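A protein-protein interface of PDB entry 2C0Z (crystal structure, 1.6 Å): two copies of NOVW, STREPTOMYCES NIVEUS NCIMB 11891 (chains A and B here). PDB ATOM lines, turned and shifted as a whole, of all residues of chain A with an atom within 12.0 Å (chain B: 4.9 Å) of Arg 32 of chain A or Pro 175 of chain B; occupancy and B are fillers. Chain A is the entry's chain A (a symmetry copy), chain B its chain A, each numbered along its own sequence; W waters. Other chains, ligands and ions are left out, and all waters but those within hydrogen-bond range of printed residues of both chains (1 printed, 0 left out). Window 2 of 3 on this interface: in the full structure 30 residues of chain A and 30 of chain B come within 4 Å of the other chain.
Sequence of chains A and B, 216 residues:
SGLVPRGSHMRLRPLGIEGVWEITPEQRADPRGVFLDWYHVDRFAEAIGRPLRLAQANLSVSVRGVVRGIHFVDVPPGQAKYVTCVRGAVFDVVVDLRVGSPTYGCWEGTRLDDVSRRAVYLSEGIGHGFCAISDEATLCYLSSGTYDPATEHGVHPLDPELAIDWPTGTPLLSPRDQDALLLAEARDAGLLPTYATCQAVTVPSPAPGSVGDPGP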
ATOM      1  N   SER A   1      37.717  -5.956  13.178  1.00  0.00           N
ATOM      2  CA  SER A   1      36.267  -5.557  13.087  1.00  0.00           C
ATOM      3  C   SER A   1      35.735  -4.800  14.314  1.00  0.00           C
ATOM      4  O   SER A   1      34.633  -4.230  14.242  1.00  0.00           O
ATOM      5  CB  SER A   1      35.417  -6.808  12.980  1.00  0.00           C
ATOM      6  OG  SER A   1      35.665  -7.534  14.159  1.00  0.00           O
ATOM      7  N   GLY A   2      36.471  -4.821  15.430  1.00  0.00           N
ATOM      8  CA  GLY A   2      35.894  -4.552  16.743  1.00  0.00           C
ATOM      9  C   GLY A   2      34.852  -5.607  17.124  1.00  0.00           C
ATOM     10  O   GLY A   2      34.596  -6.509  16.334  1.00  0.00           O
ATOM     11  N   LEU A   3      34.314  -5.553  18.348  1.00  0.00           N
ATOM     12  CA  LEU A   3      33.259  -6.493  18.758  1.00  0.00           C
ATOM     13  C   LEU A   3      32.002  -6.283  17.896  1.00  0.00           C
ATOM     14  O   LEU A   3      31.502  -5.165  17.778  1.00  0.00           O
ATOM     15  CB  LEU A   3      32.917  -6.272  20.230  1.00  0.00           C
ATOM     16  CG  LEU A   3      31.906  -7.181  20.910  1.00  0.00           C
ATOM     17  CD1 LEU A   3      32.472  -8.582  21.023  1.00  0.00           C
ATOM     18  CD2 LEU A   3      31.603  -6.625  22.280  1.00  0.00           C
ATOM     19  N   VAL A   4      31.494  -7.349  17.308  1.00  0.00           N
ATOM     20  CA  VAL A   4      30.334  -7.282  16.445  1.00  0.00           C
ATOM     21  C   VAL A   4      29.179  -7.970  17.152  1.00  0.00           C
ATOM     22  O   VAL A   4      29.237  -9.175  17.442  1.00  0.00           O
ATOM     23  CB  VAL A   4      30.606  -7.936  15.100  1.00  0.00           C
ATOM     24  CG1 VAL A   4      29.384  -7.820  14.212  1.00  0.00           C
ATOM     25  CG2 VAL A   4      31.816  -7.261  14.435  1.00  0.00           C
ATOM     26  N   PRO A   5      28.125  -7.216  17.472  1.00  0.00           N
ATOM     27  CA  PRO A   5      27.075  -7.747  18.326  1.00  0.00           C
ATOM     28  C   PRO A   5      26.164  -8.690  17.581  1.00  0.00           C
ATOM     29  O   PRO A   5      26.044  -8.667  16.369  1.00  0.00           O
ATOM     30  CB  PRO A   5      26.330  -6.496  18.765  1.00  0.00           C
ATOM     31  CG  PRO A   5      26.430  -5.622  17.638  1.00  0.00           C
ATOM     32  CD  PRO A   5      27.855  -5.825  17.061  1.00  0.00           C
ATOM     33  N   GLN A  27      17.981  -6.145  16.170  1.00  0.00           N
ATOM     34  CA  GLN A  27      19.331  -5.624  15.926  1.00  0.00           C
ATOM     35  C   GLN A  27      19.990  -6.340  14.745  1.00  0.00           C
ATOM     36  O   GLN A  27      19.861  -7.559  14.603  1.00  0.00           O
ATOM     37  CB  GLN A  27      20.173  -5.858  17.192  1.00  0.00           C
ATOM     38  CG  GLN A  27      21.658  -5.420  17.092  1.00  0.00           C
ATOM     39  CD  GLN A  27      22.322  -5.278  18.454  1.00  0.00           C
ATOM     40  OE1 GLN A  27      22.480  -4.161  18.943  1.00  0.00           O
ATOM     41  NE2 GLN A  27      22.705  -6.386  19.064  1.00  0.00           N
ATOM     42  N   ARG A  28      20.682  -5.564  13.912  1.00  0.00           N
ATOM     43  CA  ARG A  28      21.514  -6.064  12.853  1.00  0.00           C
ATOM     44  C   ARG A  28      22.825  -5.318  12.856  1.00  0.00           C
ATOM     45  O   ARG A  28      22.906  -4.152  13.285  1.00  0.00           O
ATOM     46  CB  ARG A  28      20.866  -5.925  11.485  1.00  0.00           C
ATOM     47  CG  ARG A  28      20.639  -4.561  10.966  1.00  0.00           C
ATOM     48  CD  ARG A  28      19.981  -4.546   9.555  1.00  0.00           C
ATOM     49  NE  ARG A  28      19.953  -3.183   9.004  1.00  0.00           N
ATOM     50  CZ  ARG A  28      18.860  -2.429   8.835  1.00  0.00           C
ATOM     51  NH1 ARG A  28      17.649  -2.875   9.167  1.00  0.00           N
ATOM     52  NH2 ARG A  28      18.974  -1.205   8.319  1.00  0.00           N
ATOM     53  N   ALA A  29      23.855  -5.994  12.353  1.00  0.00           N
ATOM     54  CA  ALA A  29      25.142  -5.350  12.169  1.00  0.00           C
ATOM     55  C   ALA A  29      25.688  -5.607  10.737  1.00  0.00           C
ATOM     56  O   ALA A  29      25.413  -6.652  10.125  1.00  0.00           O
ATOM     57  CB  ALA A  29      26.083  -5.820  13.219  1.00  0.00           C
ATOM     58  N   ASP A  30      26.409  -4.630  10.187  1.00  0.00           N
ATOM     59  CA  ASP A  30      27.155  -4.803   8.913  1.00  0.00           C
ATOM     60  C   ASP A  30      28.465  -4.019   8.989  1.00  0.00           C
ATOM     61  O   ASP A  30      28.746  -3.419   9.988  1.00  0.00           O
ATOM     62  CB  ASP A  30      26.265  -4.412   7.725  1.00  0.00           C
ATOM     63  CG  ASP A  30      25.925  -2.931   7.684  1.00  0.00           C
ATOM     64  OD1 ASP A  30      26.746  -2.081   8.081  1.00  0.00           O
ATOM     65  OD2 ASP A  30      24.838  -2.529   7.232  1.00  0.00           O
ATOM     66  N   PRO A  31      29.342  -4.063   7.989  1.00  0.00           N
ATOM     67  CA  PRO A  31      30.648  -3.387   8.151  1.00  0.00           C
ATOM     68  C   PRO A  31      30.588  -1.865   8.436  1.00  0.00           C
ATOM     69  O   PRO A  31      31.534  -1.263   8.963  1.00  0.00           O
ATOM     70  CB  PRO A  31      31.365  -3.671   6.818  1.00  0.00           C
ATOM     71  CG  PRO A  31      30.645  -4.907   6.251  1.00  0.00           C
ATOM     72  CD  PRO A  31      29.217  -4.766   6.695  1.00  0.00           C
ATOM     73  N   ARG A  32      29.496  -1.213   8.092  1.00  0.00           N
ATOM     74  CA  ARG A  32      29.390   0.213   8.397  1.00  0.00           C
ATOM     75  C   ARG A  32      28.911   0.524   9.828  1.00  0.00           C
ATOM     76  O   ARG A  32      29.096   1.636  10.293  1.00  0.00           O
ATOM     77  CB  ARG A  32      28.504   0.909   7.344  1.00  0.00           C
ATOM     78  CG  ARG A  32      29.171   0.978   5.952  1.00  0.00           C
ATOM     79  CD  ARG A  32      28.208   1.312   4.796  1.00  0.00           C
ATOM     80  NE  ARG A  32      27.184   0.279   4.643  1.00  0.00           N
ATOM     81  CZ  ARG A  32      27.395  -0.913   4.080  1.00  0.00           C
ATOM     82  NH1 ARG A  32      28.584  -1.228   3.592  1.00  0.00           N
ATOM     83  NH2 ARG A  32      26.405  -1.792   3.986  1.00  0.00           N
ATOM     84  N   GLY A  33      28.303  -0.445  10.512  1.00  0.00           N
ATOM     85  CA  GLY A  33      27.750  -0.193  11.819  1.00  0.00           C
ATOM     86  C   GLY A  33      26.675  -1.158  12.296  1.00  0.00           C
ATOM     87  O   GLY A  33      26.595  -2.331  11.892  1.00  0.00           O
ATOM     88  N   VAL A  34      25.880  -0.647  13.221  1.00  0.00           N
ATOM     89  CA  VAL A  34      24.860  -1.429  13.908  1.00  0.00           C
ATOM     90  C   VAL A  34      23.581  -0.626  13.858  1.00  0.00           C
ATOM     91  O   VAL A  34      23.618   0.586  14.009  1.00  0.00           O
ATOM     92  CB  VAL A  34      25.277  -1.652  15.363  1.00  0.00           C
ATOM     93  CG1 VAL A  34      24.245  -2.480  16.116  1.00  0.00           C
ATOM     94  CG2 VAL A  34      26.625  -2.332  15.436  1.00  0.00           C
ATOM     95  N   PHE A  35      22.463  -1.302  13.628  1.00  0.00           N
ATOM     96  CA  PHE A  35      21.151  -0.683  13.627  1.00  0.00           C
ATOM     97  C   PHE A  35      20.186  -1.496  14.433  1.00  0.00           C
ATOM     98  O   PHE A  35      20.089  -2.711  14.279  1.00  0.00           O
ATOM     99  CB  PHE A  35      20.629  -0.532  12.205  1.00  0.00           C
ATOM    100  CG  PHE A  35      19.447   0.440  12.139  1.00  0.00           C
ATOM    101  CD1 PHE A  35      19.614   1.795  12.361  1.00  0.00           C
ATOM    102  CD2 PHE A  35      18.154  -0.043  11.966  1.00  0.00           C
ATOM    103  CE1 PHE A  35      18.515   2.674  12.360  1.00  0.00           C
ATOM    104  CE2 PHE A  35      17.045   0.821  11.947  1.00  0.00           C
ATOM    105  CZ  PHE A  35      17.220   2.173  12.146  1.00  0.00           C
ATOM    106  N   LEU A  36      19.452  -0.826  15.291  1.00  0.00           N
ATOM    107  CA  LEU A  36      18.462  -1.527  16.076  1.00  0.00           C
ATOM    108  C   LEU A  36      17.209  -0.737  16.359  1.00  0.00           C
ATOM    109  O   LEU A  36      17.226   0.480  16.442  1.00  0.00           O
ATOM    110  CB  LEU A  36      19.071  -2.017  17.383  1.00  0.00           C
ATOM    111  CG  LEU A  36      19.700  -0.985  18.299  1.00  0.00           C
ATOM    112  CD1 LEU A  36      19.499  -1.409  19.742  1.00  0.00           C
ATOM    113  CD2 LEU A  36      21.203  -0.768  17.963  1.00  0.00           C
ATOM    114  N   ARG A 117      22.303  -4.451  24.325  1.00  0.00           N
ATOM    115  CA  ARG A 117      21.393  -3.334  24.127  1.00  0.00           C
ATOM    116  C   ARG A 117      19.923  -3.631  24.470  1.00  0.00           C
ATOM    117  O   ARG A 117      18.975  -3.171  23.791  1.00  0.00           O
ATOM    118  CB  ARG A 117      21.538  -2.797  22.710  1.00  0.00           C
ATOM    119  CG  ARG A 117      22.914  -2.213  22.443  1.00  0.00           C
ATOM    120  CD  ARG A 117      22.989  -1.403  21.150  1.00  0.00           C
ATOM    121  NE  ARG A 117      24.333  -0.880  20.841  1.00  0.00           N
ATOM    122  CZ  ARG A 117      24.810   0.283  21.246  1.00  0.00           C
ATOM    123  NH1 ARG A 117      24.073   1.131  21.948  1.00  0.00           N
ATOM    124  NH2 ARG A 117      26.051   0.620  20.906  1.00  0.00           N
ATOM    125  N   VAL B  61      24.720   2.907  15.090  1.00  0.00           N
ATOM    126  CA  VAL B  61      26.135   3.102  15.382  1.00  0.00           C
ATOM    127  C   VAL B  61      26.840   3.088  14.044  1.00  0.00           C
ATOM    128  O   VAL B  61      26.616   2.193  13.254  1.00  0.00           O
ATOM    129  CB  VAL B  61      26.707   1.975  16.281  1.00  0.00           C
ATOM    130  CG1 VAL B  61      28.165   2.251  16.568  1.00  0.00           C
ATOM    131  CG2 VAL B  61      25.900   1.855  17.547  1.00  0.00           C
ATOM    132  N   SER B  62      27.615   4.114  13.751  1.00  0.00           N
ATOM    133  CA  SER B  62      28.266   4.242  12.452  1.00  0.00           C
ATOM    134  C   SER B  62      29.714   4.590  12.633  1.00  0.00           C
ATOM    135  O   SER B  62      30.057   5.334  13.516  1.00  0.00           O
ATOM    136  CB  SER B  62      27.627   5.369  11.653  1.00  0.00           C
ATOM    137  OG  SER B  62      26.276   5.138  11.541  1.00  0.00           O
ATOM    138  N   VAL B  63      30.547   4.066  11.748  1.00  0.00           N
ATOM    139  CA  VAL B  63      31.955   4.448  11.732  1.00  0.00           C
ATOM    140  C   VAL B  63      32.204   5.792  11.020  1.00  0.00           C
ATOM    141  O   VAL B  63      31.441   6.229  10.168  1.00  0.00           O
ATOM    142  CB  VAL B  63      32.821   3.304  11.143  1.00  0.00           C
ATOM    143  CG1 VAL B  63      32.528   1.989  11.841  1.00  0.00           C
ATOM    144  CG2 VAL B  63      32.586   3.140   9.694  1.00  0.00           C
ATOM    145  N   VAL B  66      31.133   7.377   7.351  1.00  0.00           N
ATOM    146  CA  VAL B  66      29.881   6.820   6.832  1.00  0.00           C
ATOM    147  C   VAL B  66      28.929   7.993   6.570  1.00  0.00           C
ATOM    148  O   VAL B  66      28.776   8.819   7.444  1.00  0.00           O
ATOM    149  CB  VAL B  66      29.221   5.901   7.891  1.00  0.00           C
ATOM    150  CG1 VAL B  66      27.669   5.830   7.698  1.00  0.00           C
ATOM    151  CG2 VAL B  66      29.881   4.506   7.897  1.00  0.00           C
ATOM    152  N   LEU B 172      31.507   6.977   2.977  1.00  0.00           N
ATOM    153  CA  LEU B 172      31.197   5.563   2.878  1.00  0.00           C
ATOM    154  C   LEU B 172      29.674   5.424   2.793  1.00  0.00           C
ATOM    155  O   LEU B 172      28.973   5.632   3.805  1.00  0.00           O
ATOM    156  CB  LEU B 172      31.739   4.793   4.092  1.00  0.00           C
ATOM    157  N   LEU B 173      29.194   5.042   1.604  1.00  0.00           N
ATOM    158  CA  LEU B 173      27.765   4.848   1.314  1.00  0.00           C
ATOM    159  C   LEU B 173      27.421   3.371   1.238  1.00  0.00           C
ATOM    160  O   LEU B 173      28.185   2.573   0.680  1.00  0.00           O
ATOM    161  CB  LEU B 173      27.403   5.493  -0.043  1.00  0.00           C
ATOM    162  CG  LEU B 173      27.023   6.972  -0.104  1.00  0.00           C
ATOM    163  CD1 LEU B 173      27.844   7.831   0.787  1.00  0.00           C
ATOM    164  CD2 LEU B 173      27.061   7.460  -1.539  1.00  0.00           C
ATOM    165  N   SER B 174      26.255   3.007   1.757  1.00  0.00           N
ATOM    166  CA  SER B 174      25.692   1.682   1.605  1.00  0.00           C
ATOM    167  C   SER B 174      25.233   1.521   0.154  1.00  0.00           C
ATOM    168  O   SER B 174      25.019   2.521  -0.528  1.00  0.00           O
ATOM    169  CB  SER B 174      24.487   1.521   2.514  1.00  0.00           C
ATOM    170  OG  SER B 174      23.431   2.382   2.077  1.00  0.00           O
ATOM    171  N   PRO B 175      25.063   0.293  -0.320  1.00  0.00           N
ATOM    172  CA  PRO B 175      24.561   0.090  -1.682  1.00  0.00           C
ATOM    173  C   PRO B 175      23.235   0.821  -1.907  1.00  0.00           C
ATOM    174  O   PRO B 175      23.051   1.468  -2.951  1.00  0.00           O
ATOM    175  CB  PRO B 175      24.419  -1.445  -1.777  1.00  0.00           C
ATOM    176  CG  PRO B 175      25.407  -1.963  -0.794  1.00  0.00           C
ATOM    177  CD  PRO B 175      25.386  -0.986   0.355  1.00  0.00           C
ATOM    178  N   ARG B 176      22.352   0.783  -0.914  1.00  0.00           N
ATOM    179  CA  ARG B 176      21.065   1.469  -0.996  1.00  0.00           C
ATOM    180  C   ARG B 176      21.275   2.955  -1.321  1.00  0.00           C
ATOM    181  O   ARG B 176      20.622   3.488  -2.206  1.00  0.00           O
ATOM    182  CB  ARG B 176      20.289   1.310   0.300  1.00  0.00           C
ATOM    183  CG  ARG B 176      19.149   2.268   0.478  1.00  0.00           C
ATOM    184  CD  ARG B 176      18.574   2.381   1.873  1.00  0.00           C
ATOM    185  NE  ARG B 176      17.492   3.370   1.864  1.00  0.00           N
ATOM    186  CZ  ARG B 176      16.675   3.605   2.881  1.00  0.00           C
ATOM    187  NH1 ARG B 176      16.812   2.925   4.012  1.00  0.00           N
ATOM    188  NH2 ARG B 176      15.719   4.527   2.765  1.00  0.00           N
ATOM    189  N   ASP B 177      22.142   3.641  -0.586  1.00  0.00           N
ATOM    190  CA  ASP B 177      22.295   5.083  -0.793  1.00  0.00           C
ATOM    191  C   ASP B 177      23.099   5.415  -2.056  1.00  0.00           C
ATOM    192  O   ASP B 177      22.845   6.420  -2.705  1.00  0.00           O
ATOM    193  CB  ASP B 177      22.897   5.742   0.451  1.00  0.00           C
ATOM    194  CG  ASP B 177      21.982   5.673   1.637  1.00  0.00           C
ATOM    195  OD1 ASP B 177      20.745   5.540   1.449  1.00  0.00           O
ATOM    196  OD2 ASP B 177      22.406   5.736   2.832  1.00  0.00           O
ATOM    197  N   GLN B 178      24.020   4.530  -2.432  1.00  0.00           N
ATOM    198  CA  GLN B 178      24.792   4.691  -3.666  1.00  0.00           C
ATOM    199  C   GLN B 178      23.858   4.614  -4.873  1.00  0.00           C
ATOM    200  O   GLN B 178      24.077   5.300  -5.869  1.00  0.00           O
ATOM    201  CB  GLN B 178      25.847   3.579  -3.801  1.00  0.00           C
ATOM    202  CG  GLN B 178      27.057   3.694  -2.934  1.00  0.00           C
ATOM    203  CD  GLN B 178      28.055   2.547  -3.178  1.00  0.00           C
ATOM    204  OE1 GLN B 178      28.398   2.257  -4.325  1.00  0.00           O
ATOM    205  NE2 GLN B 178      28.513   1.909  -2.107  1.00  0.00           N
ATOM    206  N   ASP B 179      22.824   3.788  -4.763  1.00  0.00           N
ATOM    207  CA  ASP B 179      21.914   3.497  -5.877  1.00  0.00           C
ATOM    208  C   ASP B 179      20.664   4.387  -5.886  1.00  0.00           C
ATOM    209  O   ASP B 179      19.823   4.291  -6.779  1.00  0.00           O
ATOM    210  CB  ASP B 179      21.480   2.027  -5.838  1.00  0.00           C
ATOM    211  CG  ASP B 179      22.631   1.071  -6.120  1.00  0.00           C
ATOM    212  OD1 ASP B 179      23.704   1.503  -6.601  1.00  0.00           O
ATOM    213  OD2 ASP B 179      22.543  -0.139  -5.869  1.00  0.00           O
HETATM  214  O   HOH W   1      26.302   3.030   9.927  1.00  0.00           O
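The backbone carbonyl oxygen of Val 34 of chain A is in hydrogen-bond range of the backbone NH of Val 61 of chain B (2.8 Å). N of Val 63 of chain B is in hydrogen-bond range of O of Arg 32 of chain A.
OG of Ser 174 of chain B sits at hydrogen-bond distance from N of Asp 177 of chain B, 3.2 Å away. The side-chain carboxylate (OD2) of Asp 30 of chain A is in salt-bridge range of the guanidinium group (NH2) of Arg 32 of chain A. The side-chain carboxylate (OD1) of Asp 30 of chain A lies within hydrogen-bond range of the backbone NH (N) of Gly 33 of chain A, 3.3 Å away.
Arg 32 of chain A touches Val 61 of chain B. CA of Ser 62 of chain B touches O of Arg 32 of chain A (3.5 Å). O of Arg 32 of chain A touches CG2 of Val 66 of chain B, 3.8 Å away. Arg 32 of chain A touches Ser 174 of chain B. NH2 of Arg 32 of chain A touches CD of Pro 175 of chain B (3.9 Å). O of Val 61 of chain B touches CA of Gly 33 of chain A, 3.0 Å away. Val 61 of chain B touches Arg 117 of chain A.
Of chain B, only Val 61, Ser 62, Val 63, Val 66, Ser 174 and Pro 175 come within 4 Å of Arg 32 of chain A. Printed residues of chain B within 4 Å of Gly 33 of chain A: Val 61 (3.0 Å). Printed residues of chain B within 4 Å of Val 34 of chain A: Val 61. Of the printed residues of chain B, Arg 117 of chain A touches Val 61 (3.6 Å). Of the printed residues of chain A, Val 61 of chain B touches Arg 32 (3.9 Å), Gly 33 (3.0 Å), Val 34 (2.8 Å) and Arg 117 (3.6 Å). Ser 62 of chain B touches just one residue of chain A: Arg 32 (3.5 Å). Val 63 of chain B touches one residue of chain A. No residue of chain A comes within 4 Å of Leu 172 of chain B. No residue of chain A comes within 4 Å of Leu 173 of chain B. Pro 175 of chain B touches just one residue of chain A: Arg 32. No residue of chain A comes within 4 Å of Asp 177 of chain B. No residue of chain A comes within 4 Å of Gln 178 of chain B. Asp 179 of chain B touches none of the printed residues of chain A. The nearest residue of chain B that does not touch Arg 32 of chain A is Leu 173 of chain B (4.2 Å). The nearest residue of chain A that does not touch Pro 175 of chain B is Asp 30 of chain A (7.1 Å).
No position is printed for both chains. Of the 9 pairs that touch across the chains among the printed residues, none has its exchanged pair printed and touching as well.
Water W1 lies within hydrogen-bond range of OG of Ser 62 of chain B (2.7 Å), O of Arg 32 of chain A (3.1 Å) and O of Val 61 of chain B (3.4 Å).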
